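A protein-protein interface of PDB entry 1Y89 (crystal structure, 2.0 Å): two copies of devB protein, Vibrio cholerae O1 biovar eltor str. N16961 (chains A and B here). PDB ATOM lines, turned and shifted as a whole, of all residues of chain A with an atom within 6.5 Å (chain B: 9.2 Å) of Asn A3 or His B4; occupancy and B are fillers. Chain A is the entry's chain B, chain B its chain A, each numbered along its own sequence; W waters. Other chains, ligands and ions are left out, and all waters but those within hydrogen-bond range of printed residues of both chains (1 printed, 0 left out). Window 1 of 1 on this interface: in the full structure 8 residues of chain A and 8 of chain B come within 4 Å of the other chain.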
ATOM      1  N   MET A   1      30.446   8.856 -21.095  1.00  0.00           N
ATOM      2  CA  MET A   1      29.707  10.029 -20.546  1.00  0.00           C
ATOM      3  C   MET A   1      30.677  11.048 -19.894  1.00  0.00           C
ATOM      4  O   MET A   1      31.653  10.668 -19.246  1.00  0.00           O
ATOM      5  CB  MET A   1      28.625   9.505 -19.597  1.00  0.00           C
ATOM      6  CG  MET A   1      27.556  10.490 -19.169  1.00  0.00           C
ATOM      7  SD  MET A   1      28.132  11.419 -17.476  1.00  0.00           S
ATOM      8  CE  MET A   1      28.075   9.895 -16.324  1.00  0.00           C
ATOM      9  N   ILE A   2      30.423  12.335 -20.096  1.00  0.00           N
ATOM     10  CA  ILE A   2      31.175  13.395 -19.423  1.00  0.00           C
ATOM     11  C   ILE A   2      30.252  14.214 -18.507  1.00  0.00           C
ATOM     12  O   ILE A   2      29.121  14.541 -18.886  1.00  0.00           O
ATOM     13  CB  ILE A   2      31.948  14.306 -20.412  1.00  0.00           C
ATOM     14  CG1 ILE A   2      32.736  15.411 -19.682  1.00  0.00           C
ATOM     15  CG2 ILE A   2      31.043  14.878 -21.473  1.00  0.00           C
ATOM     16  CD1 ILE A   2      33.998  15.837 -20.439  1.00  0.00           C
ATOM     17  N   ASN A   3      30.750  14.523 -17.313  1.00  0.00           N
ATOM     18  CA  ASN A   3      29.994  15.231 -16.262  1.00  0.00           C
ATOM     19  C   ASN A   3      30.834  16.396 -15.762  1.00  0.00           C
ATOM     20  O   ASN A   3      31.960  16.200 -15.316  1.00  0.00           O
ATOM     21  CB  ASN A   3      29.672  14.218 -15.160  1.00  0.00           C
ATOM     22  CG  ASN A   3      28.733  14.748 -14.057  1.00  0.00           C
ATOM     23  OD1 ASN A   3      28.660  14.132 -12.995  1.00  0.00           O
ATOM     24  ND2 ASN A   3      28.030  15.855 -14.287  1.00  0.00           N
ATOM     25  N   HIS A   4      30.346  17.618 -15.938  1.00  0.00           N
ATOM     26  CA  HIS A   4      31.032  18.771 -15.408  1.00  0.00           C
ATOM     27  C   HIS A   4      30.214  19.279 -14.220  1.00  0.00           C
ATOM     28  O   HIS A   4      29.001  19.486 -14.373  1.00  0.00           O
ATOM     29  CB  HIS A   4      31.116  19.899 -16.435  1.00  0.00           C
ATOM     30  CG  HIS A   4      31.682  19.499 -17.767  1.00  0.00           C
ATOM     31  ND1 HIS A   4      32.782  20.121 -18.320  1.00  0.00           N
ATOM     32  CD2 HIS A   4      31.264  18.593 -18.684  1.00  0.00           C
ATOM     33  CE1 HIS A   4      33.029  19.604 -19.510  1.00  0.00           C
ATOM     34  NE2 HIS A   4      32.127  18.668 -19.753  1.00  0.00           N
ATOM     35  N   LYS A   5      30.865  19.527 -13.079  1.00  0.00           N
ATOM     36  CA  LYS A   5      30.165  20.023 -11.886  1.00  0.00           C
ATOM     37  C   LYS A   5      30.817  21.314 -11.446  1.00  0.00           C
ATOM     38  O   LYS A   5      32.036  21.363 -11.233  1.00  0.00           O
ATOM     39  CB  LYS A   5      30.246  18.994 -10.777  1.00  0.00           C
ATOM     40  CG  LYS A   5      29.761  17.588 -11.198  1.00  0.00           C
ATOM     41  CD  LYS A   5      29.769  16.653  -9.984  1.00  0.00           C
ATOM     42  CE  LYS A   5      28.841  15.471 -10.166  1.00  0.00           C
ATOM     43  NZ  LYS A   5      27.977  15.381  -8.929  1.00  0.00           N
ATOM     44  N   ILE A   6      30.022  22.368 -11.304  1.00  0.00           N
ATOM     45  CA  ILE A   6      30.589  23.628 -10.819  1.00  0.00           C
ATOM     46  C   ILE A   6      29.960  23.939  -9.484  1.00  0.00           C
ATOM     47  O   ILE A   6      28.732  24.090  -9.385  1.00  0.00           O
ATOM     48  CB  ILE A   6      30.400  24.809 -11.814  1.00  0.00           C
ATOM     49  CG1 ILE A   6      31.047  24.475 -13.185  1.00  0.00           C
ATOM     50  CG2 ILE A   6      31.000  26.123 -11.213  1.00  0.00           C
ATOM     51  CD1 ILE A   6      30.900  25.643 -14.225  1.00  0.00           C
ATOM     52  N   VAL A 224      32.850   7.098 -16.948  1.00  0.00           N
ATOM     53  CA  VAL A 224      32.519   8.495 -16.648  1.00  0.00           C
ATOM     54  C   VAL A 224      33.800   9.314 -16.506  1.00  0.00           C
ATOM     55  O   VAL A 224      34.711   8.874 -15.813  1.00  0.00           O
ATOM     56  CB  VAL A 224      31.726   8.546 -15.294  1.00  0.00           C
ATOM     57  CG1 VAL A 224      31.484   9.949 -14.873  1.00  0.00           C
ATOM     58  CG2 VAL A 224      30.362   7.851 -15.458  1.00  0.00           C
ATOM     59  N   THR A 225      33.869  10.466 -17.189  1.00  0.00           N
ATOM     60  CA  THR A 225      34.944  11.435 -16.995  1.00  0.00           C
ATOM     61  C   THR A 225      34.302  12.688 -16.421  1.00  0.00           C
ATOM     62  O   THR A 225      33.356  13.239 -17.016  1.00  0.00           O
ATOM     63  CB  THR A 225      35.656  11.788 -18.305  1.00  0.00           C
ATOM     64  OG1 THR A 225      36.126  10.584 -18.918  1.00  0.00           O
ATOM     65  CG2 THR A 225      36.865  12.739 -18.058  1.00  0.00           C
ATOM     66  N   GLU A 226      34.823  13.136 -15.276  1.00  0.00           N
ATOM     67  CA  GLU A 226      34.228  14.257 -14.559  1.00  0.00           C
ATOM     68  C   GLU A 226      35.207  15.389 -14.408  1.00  0.00           C
ATOM     69  O   GLU A 226      36.397  15.146 -14.227  1.00  0.00           O
ATOM     70  CB  GLU A 226      33.768  13.833 -13.153  1.00  0.00           C
ATOM     71  CG  GLU A 226      32.954  12.579 -13.160  1.00  0.00           C
ATOM     72  CD  GLU A 226      32.391  12.251 -11.803  1.00  0.00           C
ATOM     73  OE1 GLU A 226      33.179  12.144 -10.846  1.00  0.00           O
ATOM     74  OE2 GLU A 226      31.168  12.063 -11.706  1.00  0.00           O
ATOM     75  N   TRP A 227      34.675  16.613 -14.421  1.00  0.00           N
ATOM     76  CA  TRP A 227      35.433  17.812 -14.122  1.00  0.00           C
ATOM     77  C   TRP A 227      34.756  18.500 -12.922  1.00  0.00           C
ATOM     78  O   TRP A 227      33.578  18.886 -13.026  1.00  0.00           O
ATOM     79  CB  TRP A 227      35.428  18.721 -15.346  1.00  0.00           C
ATOM     80  CG  TRP A 227      36.302  18.174 -16.455  1.00  0.00           C
ATOM     81  CD1 TRP A 227      35.955  17.248 -17.381  1.00  0.00           C
ATOM     82  CD2 TRP A 227      37.664  18.525 -16.716  1.00  0.00           C
ATOM     83  NE1 TRP A 227      37.027  16.984 -18.210  1.00  0.00           N
ATOM     84  CE2 TRP A 227      38.086  17.760 -17.825  1.00  0.00           C
ATOM     85  CE3 TRP A 227      38.576  19.414 -16.114  1.00  0.00           C
ATOM     86  CZ2 TRP A 227      39.381  17.858 -18.355  1.00  0.00           C
ATOM     87  CZ3 TRP A 227      39.859  19.506 -16.638  1.00  0.00           C
ATOM     88  CH2 TRP A 227      40.242  18.736 -17.746  1.00  0.00           C
ATOM     89  N   TYR A 228      35.460  18.582 -11.788  1.00  0.00           N
ATOM     90  CA  TYR A 228      34.960  19.276 -10.597  1.00  0.00           C
ATOM     91  C   TYR A 228      35.645  20.633 -10.517  1.00  0.00           C
ATOM     92  O   TYR A 228      36.867  20.676 -10.315  1.00  0.00           O
ATOM     93  CB  TYR A 228      35.299  18.509  -9.307  1.00  0.00           C
ATOM     94  CG  TYR A 228      34.426  17.313  -9.015  1.00  0.00           C
ATOM     95  CD1 TYR A 228      34.466  16.177  -9.829  1.00  0.00           C
ATOM     96  CD2 TYR A 228      33.572  17.311  -7.919  1.00  0.00           C
ATOM     97  CE1 TYR A 228      33.624  15.082  -9.566  1.00  0.00           C
ATOM     98  CE2 TYR A 228      32.765  16.233  -7.634  1.00  0.00           C
ATOM     99  CZ  TYR A 228      32.786  15.128  -8.448  1.00  0.00           C
ATOM    100  OH  TYR A 228      31.966  14.085  -8.163  1.00  0.00           O
ATOM    101  N   MET B   1      24.660  24.693  -7.097  1.00  0.00           N
ATOM    102  CA  MET B   1      25.686  24.114  -8.024  1.00  0.00           C
ATOM    103  C   MET B   1      25.061  23.797  -9.390  1.00  0.00           C
ATOM    104  O   MET B   1      23.828  23.675  -9.512  1.00  0.00           O
ATOM    105  CB  MET B   1      26.417  22.929  -7.367  1.00  0.00           C
ATOM    106  CG  MET B   1      25.641  21.646  -7.207  1.00  0.00           C
ATOM    107  SD  MET B   1      25.894  20.415  -8.783  1.00  0.00           S
ATOM    108  CE  MET B   1      26.818  18.845  -7.858  1.00  0.00           C
ATOM    109  N   ILE B   2      25.905  23.729 -10.416  1.00  0.00           N
ATOM    110  CA  ILE B   2      25.442  23.387 -11.748  1.00  0.00           C
ATOM    111  C   ILE B   2      26.146  22.118 -12.248  1.00  0.00           C
ATOM    112  O   ILE B   2      27.367  21.981 -12.111  1.00  0.00           O
ATOM    113  CB  ILE B   2      25.556  24.582 -12.742  1.00  0.00           C
ATOM    114  CG1 ILE B   2      25.058  24.182 -14.144  1.00  0.00           C
ATOM    115  CG2 ILE B   2      26.990  25.086 -12.853  1.00  0.00           C
ATOM    116  CD1 ILE B   2      24.483  25.366 -14.946  1.00  0.00           C
ATOM    117  N   ASN B   3      25.354  21.206 -12.798  1.00  0.00           N
ATOM    118  CA  ASN B   3      25.820  19.907 -13.281  1.00  0.00           C
ATOM    119  C   ASN B   3      25.464  19.776 -14.762  1.00  0.00           C
ATOM    120  O   ASN B   3      24.305  19.893 -15.133  1.00  0.00           O
ATOM    121  CB  ASN B   3      25.114  18.853 -12.422  1.00  0.00           C
ATOM    122  CG  ASN B   3      25.658  17.461 -12.579  1.00  0.00           C
ATOM    123  OD1 ASN B   3      26.749  17.231 -13.113  1.00  0.00           O
ATOM    124  ND2 ASN B   3      24.899  16.497 -12.058  1.00  0.00           N
ATOM    125  N   HIS B   4      26.459  19.622 -15.631  1.00  0.00           N
ATOM    126  CA  HIS B   4      26.210  19.356 -17.051  1.00  0.00           C
ATOM    127  C   HIS B   4      26.616  17.920 -17.341  1.00  0.00           C
ATOM    128  O   HIS B   4      27.754  17.489 -16.996  1.00  0.00           O
ATOM    129  CB  HIS B   4      27.098  20.211 -17.962  1.00  0.00           C
ATOM    130  CG  HIS B   4      26.964  21.692 -17.779  1.00  0.00           C
ATOM    131  ND1 HIS B   4      27.338  22.344 -16.621  1.00  0.00           N
ATOM    132  CD2 HIS B   4      26.597  22.661 -18.652  1.00  0.00           C
ATOM    133  CE1 HIS B   4      27.160  23.647 -16.772  1.00  0.00           C
ATOM    134  NE2 HIS B   4      26.716  23.865 -17.997  1.00  0.00           N
ATOM    135  N   LYS B   5      25.725  17.186 -17.991  1.00  0.00           N
ATOM    136  CA  LYS B   5      26.010  15.804 -18.347  1.00  0.00           C
ATOM    137  C   LYS B   5      25.846  15.631 -19.849  1.00  0.00           C
ATOM    138  O   LYS B   5      24.827  16.028 -20.405  1.00  0.00           O
ATOM    139  CB  LYS B   5      25.068  14.864 -17.611  1.00  0.00           C
ATOM    140  CG  LYS B   5      25.082  15.015 -16.102  1.00  0.00           C
ATOM    141  CD  LYS B   5      24.306  13.872 -15.463  1.00  0.00           C
ATOM    142  CE  LYS B   5      24.567  13.803 -13.976  1.00  0.00           C
ATOM    143  NZ  LYS B   5      24.805  12.381 -13.634  1.00  0.00           N
ATOM    144  N   ILE B   6      26.844  15.051 -20.504  1.00  0.00           N
ATOM    145  CA  ILE B   6      26.749  14.732 -21.948  1.00  0.00           C
ATOM    146  C   ILE B   6      26.855  13.213 -22.089  1.00  0.00           C
ATOM    147  O   ILE B   6      27.853  12.621 -21.695  1.00  0.00           O
ATOM    148  CB  ILE B   6      27.842  15.455 -22.776  1.00  0.00           C
ATOM    149  CG1 ILE B   6      27.805  16.995 -22.532  1.00  0.00           C
ATOM    150  CG2 ILE B   6      27.749  15.090 -24.306  1.00  0.00           C
ATOM    151  CD1 ILE B   6      28.994  17.723 -23.131  1.00  0.00           C
ATOM    152  N   PHE B   7      25.790  12.614 -22.600  1.00  0.00           N
ATOM    153  CA  PHE B   7      25.638  11.168 -22.757  1.00  0.00           C
ATOM    154  C   PHE B   7      25.806  10.827 -24.217  1.00  0.00           C
ATOM    155  O   PHE B   7      25.496  11.645 -25.090  1.00  0.00           O
ATOM    156  CB  PHE B   7      24.229  10.722 -22.339  1.00  0.00           C
ATOM    157  CG  PHE B   7      23.925  10.902 -20.858  1.00  0.00           C
ATOM    158  CD1 PHE B   7      23.433  12.108 -20.368  1.00  0.00           C
ATOM    159  CD2 PHE B   7      24.133   9.842 -19.962  1.00  0.00           C
ATOM    160  CE1 PHE B   7      23.139  12.255 -18.998  1.00  0.00           C
ATOM    161  CE2 PHE B   7      23.862   9.992 -18.600  1.00  0.00           C
ATOM    162  CZ  PHE B   7      23.361  11.181 -18.128  1.00  0.00           C
ATOM    163  N   SER B  16      19.738   7.055 -17.114  1.00  0.00           N
ATOM    164  CA  SER B  16      20.219   7.779 -15.938  1.00  0.00           C
ATOM    165  C   SER B  16      19.030   8.334 -15.146  1.00  0.00           C
ATOM    166  O   SER B  16      18.967   8.204 -13.910  1.00  0.00           O
ATOM    167  CB  SER B  16      21.153   8.917 -16.367  1.00  0.00           C
ATOM    168  OG  SER B  16      21.618   9.590 -15.227  1.00  0.00           O
ATOM    169  N   ILE B 187      16.672  20.903 -10.569  1.00  0.00           N
ATOM    170  CA  ILE B 187      15.946  21.027 -11.825  1.00  0.00           C
ATOM    171  C   ILE B 187      16.888  20.557 -12.916  1.00  0.00           C
ATOM    172  O   ILE B 187      18.099  20.765 -12.823  1.00  0.00           O
ATOM    173  CB  ILE B 187      15.401  22.485 -12.096  1.00  0.00           C
ATOM    174  CG1 ILE B 187      16.552  23.444 -12.469  1.00  0.00           C
ATOM    175  CG2 ILE B 187      14.616  23.043 -10.841  1.00  0.00           C
ATOM    176  CD1 ILE B 187      16.083  24.932 -12.812  1.00  0.00           C
ATOM    177  N   TYR B 189      17.297  20.301 -17.079  1.00  0.00           N
ATOM    178  CA  TYR B 189      16.900  20.611 -18.453  1.00  0.00           C
ATOM    179  C   TYR B 189      17.342  19.471 -19.361  1.00  0.00           C
ATOM    180  O   TYR B 189      18.533  19.143 -19.391  1.00  0.00           O
ATOM    181  CB  TYR B 189      17.566  21.901 -18.920  1.00  0.00           C
ATOM    182  CG  TYR B 189      17.064  23.137 -18.210  1.00  0.00           C
ATOM    183  CD1 TYR B 189      15.819  23.688 -18.548  1.00  0.00           C
ATOM    184  CD2 TYR B 189      17.853  23.786 -17.229  1.00  0.00           C
ATOM    185  CE1 TYR B 189      15.335  24.821 -17.931  1.00  0.00           C
ATOM    186  CE2 TYR B 189      17.378  24.943 -16.573  1.00  0.00           C
ATOM    187  CZ  TYR B 189      16.128  25.458 -16.949  1.00  0.00           C
ATOM    188  OH  TYR B 189      15.617  26.589 -16.347  1.00  0.00           O
ATOM    189  N   VAL B 200      21.710  25.326 -27.486  1.00  0.00           N
ATOM    190  CA  VAL B 200      22.720  24.874 -26.499  1.00  0.00           C
ATOM    191  C   VAL B 200      23.985  25.746 -26.589  1.00  0.00           C
ATOM    192  O   VAL B 200      24.462  26.261 -25.564  1.00  0.00           O
ATOM    193  CB  VAL B 200      23.053  23.350 -26.641  1.00  0.00           C
ATOM    194  CG1 VAL B 200      24.352  22.965 -25.844  1.00  0.00           C
ATOM    195  CG2 VAL B 200      21.874  22.534 -26.163  1.00  0.00           C
ATOM    196  N   ILE B 203      23.234  29.424 -25.190  1.00  0.00           N
ATOM    197  CA  ILE B 203      23.148  29.428 -23.726  1.00  0.00           C
ATOM    198  C   ILE B 203      24.517  29.118 -23.090  1.00  0.00           C
ATOM    199  O   ILE B 203      24.915  29.738 -22.090  1.00  0.00           O
ATOM    200  CB  ILE B 203      22.054  28.423 -23.248  1.00  0.00           C
ATOM    201  CG1 ILE B 203      20.686  28.816 -23.846  1.00  0.00           C
ATOM    202  CG2 ILE B 203      22.041  28.271 -21.684  1.00  0.00           C
ATOM    203  CD1 ILE B 203      19.593  27.827 -23.534  1.00  0.00           C
ATOM    204  N   HIS B 204      25.235  28.161 -23.664  1.00  0.00           N
ATOM    205  CA  HIS B 204      26.555  27.793 -23.140  1.00  0.00           C
ATOM    206  C   HIS B 204      27.584  28.922 -23.114  1.00  0.00           C
ATOM    207  O   HIS B 204      28.416  28.991 -22.205  1.00  0.00           O
ATOM    208  CB  HIS B 204      27.124  26.601 -23.896  1.00  0.00           C
ATOM    209  CG  HIS B 204      28.191  25.886 -23.137  1.00  0.00           C
ATOM    210  ND1 HIS B 204      27.912  25.108 -22.030  1.00  0.00           N
ATOM    211  CD2 HIS B 204      29.528  25.834 -23.311  1.00  0.00           C
ATOM    212  CE1 HIS B 204      29.041  24.623 -21.547  1.00  0.00           C
ATOM    213  NE2 HIS B 204      30.034  25.038 -22.310  1.00  0.00           N
ATOM    214  N   THR B 205      27.508  29.822 -24.087  1.00  0.00           N
ATOM    215  CA  THR B 205      28.604  30.765 -24.353  1.00  0.00           C
ATOM    216  C   THR B 205      28.267  32.220 -24.050  1.00  0.00           C
ATOM    217  O   THR B 205      29.131  33.087 -24.107  1.00  0.00           O
ATOM    218  CB  THR B 205      29.070  30.659 -25.834  1.00  0.00           C
ATOM    219  OG1 THR B 205      27.959  30.928 -26.699  1.00  0.00           O
ATOM    220  CG2 THR B 205      29.606  29.262 -26.132  1.00  0.00           C
ATOM    221  N   VAL B 224      20.510  22.258  -7.048  1.00  0.00           N
ATOM    222  CA  VAL B 224      21.201  21.820  -8.239  1.00  0.00           C
ATOM    223  C   VAL B 224      20.437  22.196  -9.534  1.00  0.00           C
ATOM    224  O   VAL B 224      19.227  21.942  -9.641  1.00  0.00           O
ATOM    225  CB  VAL B 224      21.372  20.272  -8.170  1.00  0.00           C
ATOM    226  CG1 VAL B 224      22.076  19.734  -9.413  1.00  0.00           C
ATOM    227  CG2 VAL B 224      22.234  19.936  -6.921  1.00  0.00           C
ATOM    228  N   THR B 225      21.141  22.783 -10.502  1.00  0.00           N
ATOM    229  CA  THR B 225      20.564  22.969 -11.834  1.00  0.00           C
ATOM    230  C   THR B 225      21.375  22.071 -12.773  1.00  0.00           C
ATOM    231  O   THR B 225      22.607  22.128 -12.754  1.00  0.00           O
ATOM    232  CB  THR B 225      20.692  24.418 -12.295  1.00  0.00           C
ATOM    233  OG1 THR B 225      20.026  25.271 -11.367  1.00  0.00           O
ATOM    234  CG2 THR B 225      20.052  24.610 -13.670  1.00  0.00           C
ATOM    235  N   GLU B 226      20.700  21.266 -13.585  1.00  0.00           N
ATOM    236  CA  GLU B 226      21.390  20.333 -14.466  1.00  0.00           C
ATOM    237  C   GLU B 226      21.010  20.539 -15.903  1.00  0.00           C
ATOM    238  O   GLU B 226      19.850  20.877 -16.221  1.00  0.00           O
ATOM    239  CB  GLU B 226      21.037  18.891 -14.089  1.00  0.00           C
ATOM    240  CG  GLU B 226      21.320  18.607 -12.652  1.00  0.00           C
ATOM    241  CD  GLU B 226      20.986  17.202 -12.246  1.00  0.00           C
ATOM    242  OE1 GLU B 226      19.859  16.723 -12.533  1.00  0.00           O
ATOM    243  OE2 GLU B 226      21.870  16.589 -11.627  1.00  0.00           O
ATOM    244  N   TRP B 227      21.968  20.249 -16.772  1.00  0.00           N
ATOM    245  CA  TRP B 227      21.743  20.168 -18.195  1.00  0.00           C
ATOM    246  C   TRP B 227      22.115  18.756 -18.645  1.00  0.00           C
ATOM    247  O   TRP B 227      23.274  18.331 -18.484  1.00  0.00           O
ATOM    248  CB  TRP B 227      22.614  21.212 -18.925  1.00  0.00           C
ATOM    249  CG  TRP B 227      22.154  22.619 -18.602  1.00  0.00           C
ATOM    250  CD1 TRP B 227      22.435  23.342 -17.495  1.00  0.00           C
ATOM    251  CD2 TRP B 227      21.259  23.397 -19.382  1.00  0.00           C
ATOM    252  NE1 TRP B 227      21.783  24.566 -17.548  1.00  0.00           N
ATOM    253  CE2 TRP B 227      21.061  24.617 -18.707  1.00  0.00           C
ATOM    254  CE3 TRP B 227      20.626  23.192 -20.611  1.00  0.00           C
ATOM    255  CZ2 TRP B 227      20.244  25.632 -19.214  1.00  0.00           C
ATOM    256  CZ3 TRP B 227      19.807  24.215 -21.119  1.00  0.00           C
ATOM    257  CH2 TRP B 227      19.623  25.403 -20.413  1.00  0.00           C
ATOM    258  N   TYR B 228      21.141  18.019 -19.169  1.00  0.00           N
ATOM    259  CA  TYR B 228      21.372  16.650 -19.670  1.00  0.00           C
ATOM    260  C   TYR B 228      21.364  16.743 -21.196  1.00  0.00           C
ATOM    261  O   TYR B 228      20.329  17.087 -21.775  1.00  0.00           O
ATOM    262  CB  TYR B 228      20.212  15.722 -19.253  1.00  0.00           C
ATOM    263  CG  TYR B 228      20.320  15.161 -17.841  1.00  0.00           C
ATOM    264  CD1 TYR B 228      20.389  16.001 -16.742  1.00  0.00           C
ATOM    265  CD2 TYR B 228      20.341  13.793 -17.615  1.00  0.00           C
ATOM    266  CE1 TYR B 228      20.514  15.481 -15.461  1.00  0.00           C
ATOM    267  CE2 TYR B 228      20.461  13.260 -16.348  1.00  0.00           C
ATOM    268  CZ  TYR B 228      20.558  14.116 -15.270  1.00  0.00           C
ATOM    269  OH  TYR B 228      20.723  13.604 -14.008  1.00  0.00           O
ATOM    270  N   LEU B 229      22.494  16.467 -21.845  1.00  0.00           N
ATOM    271  CA  LEU B 229      22.533  16.544 -23.301  1.00  0.00           C
ATOM    272  C   LEU B 229      22.956  15.197 -23.859  1.00  0.00           C
ATOM    273  O   LEU B 229      23.613  14.414 -23.165  1.00  0.00           O
ATOM    274  CB  LEU B 229      23.583  17.574 -23.764  1.00  0.00           C
ATOM    275  CG  LEU B 229      23.588  19.005 -23.197  1.00  0.00           C
ATOM    276  CD1 LEU B 229      24.621  19.819 -23.955  1.00  0.00           C
ATOM    277  CD2 LEU B 229      22.272  19.710 -23.210  1.00  0.00           C
ATOM    278  N   ALA B 234      25.012  18.441 -27.960  1.00  0.00           N
ATOM    279  CA  ALA B 234      26.284  19.038 -27.513  1.00  0.00           C
ATOM    280  C   ALA B 234      27.261  19.325 -28.648  1.00  0.00           C
ATOM    281  O   ALA B 234      28.362  19.846 -28.397  1.00  0.00           O
ATOM    282  CB  ALA B 234      26.983  18.107 -26.489  1.00  0.00           C
ATOM    283  N   ILE B 237      29.438  22.462 -28.827  1.00  0.00           N
ATOM    284  CA  ILE B 237      30.209  22.863 -27.645  1.00  0.00           C
ATOM    285  C   ILE B 237      31.175  21.788 -27.146  1.00  0.00           C
ATOM    286  O   ILE B 237      32.028  22.056 -26.306  1.00  0.00           O
ATOM    287  CB  ILE B 237      29.304  23.330 -26.488  1.00  0.00           C
ATOM    288  CG1 ILE B 237      28.392  22.194 -25.993  1.00  0.00           C
ATOM    289  CG2 ILE B 237      28.461  24.542 -26.930  1.00  0.00           C
ATOM    290  CD1 ILE B 237      27.762  22.469 -24.581  1.00  0.00           C
HETATM  291  O   HOH W   1      26.036  13.338 -10.692  1.00  0.00           O
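Ile A2 touches Lys B5, and with the chains exchanged Lys A5 touches Ile B2. Ile A2 touches Ile B6, and with the chains exchanged Ile A6 touches Ile B2. Asn A3 touches Lys B5, and with the chains exchanged Lys A5 touches Asn B3. Lys A5 touches Met B1, but with the chains exchanged Met A1 does not touch Lys B5 (4.6 Å). Positions printed for both chains: 1, 2, 3, 4, 5, 6, 224, 225, 226, 227 and 228.
Hydrophobic or aromatic side chains of chain B within 4 Å of the printed part of chain A: Met B1, Ile B2, His B4, Ile B6 and Phe B7. Of the 11 printed residues of chain A, 6 touch a printed residue of chain B. Printed residues of chain A that touch a printed residue of chain B: Met A1, Ile A2, Asn A3, His A4, Lys A5 and Ile A6. Along chain A the printed residues that touch a printed residue of chain B span positions 1 to 6. Among the printed residues, no Asp or Glu carboxylate lies within 4 Å of a Lys or Arg side-chain nitrogen of the other chain.
CG of Met A1 touches O of Ile B6 (3.3 Å). CD2 of Phe B7 touches CG of Met A1 (3.6 Å). His B4 touches Ile A2. Ile A2 touches Lys B5 (O to CA, 3.4 Å). Lys B5 touches Asn A3. Ile B2 touches His A4 (O to O, 3.7 Å). CE of Met B1 touches NZ of Lys A5, 3.8 Å away. Ile B2 touches Lys A5 (O to CA, 3.4 Å). CG of Lys A5 touches OD1 of Asn B3, at 3.6 Å. Ile A6 touches Met B1 (O to CB, 3.3 Å).
Water W1 lies within hydrogen-bond range of the side-chain amino group of Lys A5 (3.3 Å) and the side-chain amino group of Lys B5 (3.3 Å).
The backbone carbonyl oxygen (O) of Ile B2 is in hydrogen-bond range of the backbone NH (N) of Ile A6 (2.8 Å). OD1 of Asn B3 sits close to O of His A4. O of His B4 sits at hydrogen-bond distance from ND2 of Asn A3. The backbone NH of His A4 lies within hydrogen-bond range of the backbone carbonyl oxygen of His B4, 2.8 Å away. The backbone carbonyl oxygen (O) of Ile A2 is in hydrogen-bond range of the backbone NH (N) of Ile B6, at 2.8 Å. The side-chain amide nitrogen (ND2) of Asn A3 sits close to the side-chain amide oxygen (OD1) of Asn B3 (2.2 Å).
Asn A3 touches three residues of chain B. Of chain A, only Ile A2 (3.8 Å), Asn A3 (3.2 Å) and His A4 (2.8 Å) come within 4 Å of His B4. Ile A2 touches just these residues of chain B: His B4, Lys B5 and Ile B6. Printed residues of chain B within 4 Å of Ile A6: Met B1 (3.3 Å) and Ile B2 (2.8 Å). Of the printed residues of chain A, Asn B3 touches Asn A3 (2.2 Å), His A4 (3.4 Å) and Lys A5 (3.6 Å). Val B200 touches none of the printed residues of chain A. Thr B205 touches none of the printed residues of chain A. The nearest residue of chain B that does not touch Asn A3 is Ile B6 (5.1 Å). The nearest residue of chain A that does not touch His B4 is Ile A6 (4.9 Å).
The backbone carbonyl oxygen (O) of Met B1 sits at hydrogen-bond distance from the backbone NH (N) of Thr B225, 3.0 Å away. The backbone NH (N) of Asn B3 lies within hydrogen-bond range of the backbone carbonyl oxygen (O) of Thr B225 (2.9 Å). N of Lys B5 lies within hydrogen-bond range of O of Trp B227, 2.7 Å away. O of Met A1 is in hydrogen-bond range of N of Thr A225. The side-chain amide oxygen of Asn A3 lies close to the side-chain carboxylate of Glu A226. The backbone NH of Trp A227 sits at hydrogen-bond distance from the backbone carbonyl oxygen of Asn A3.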
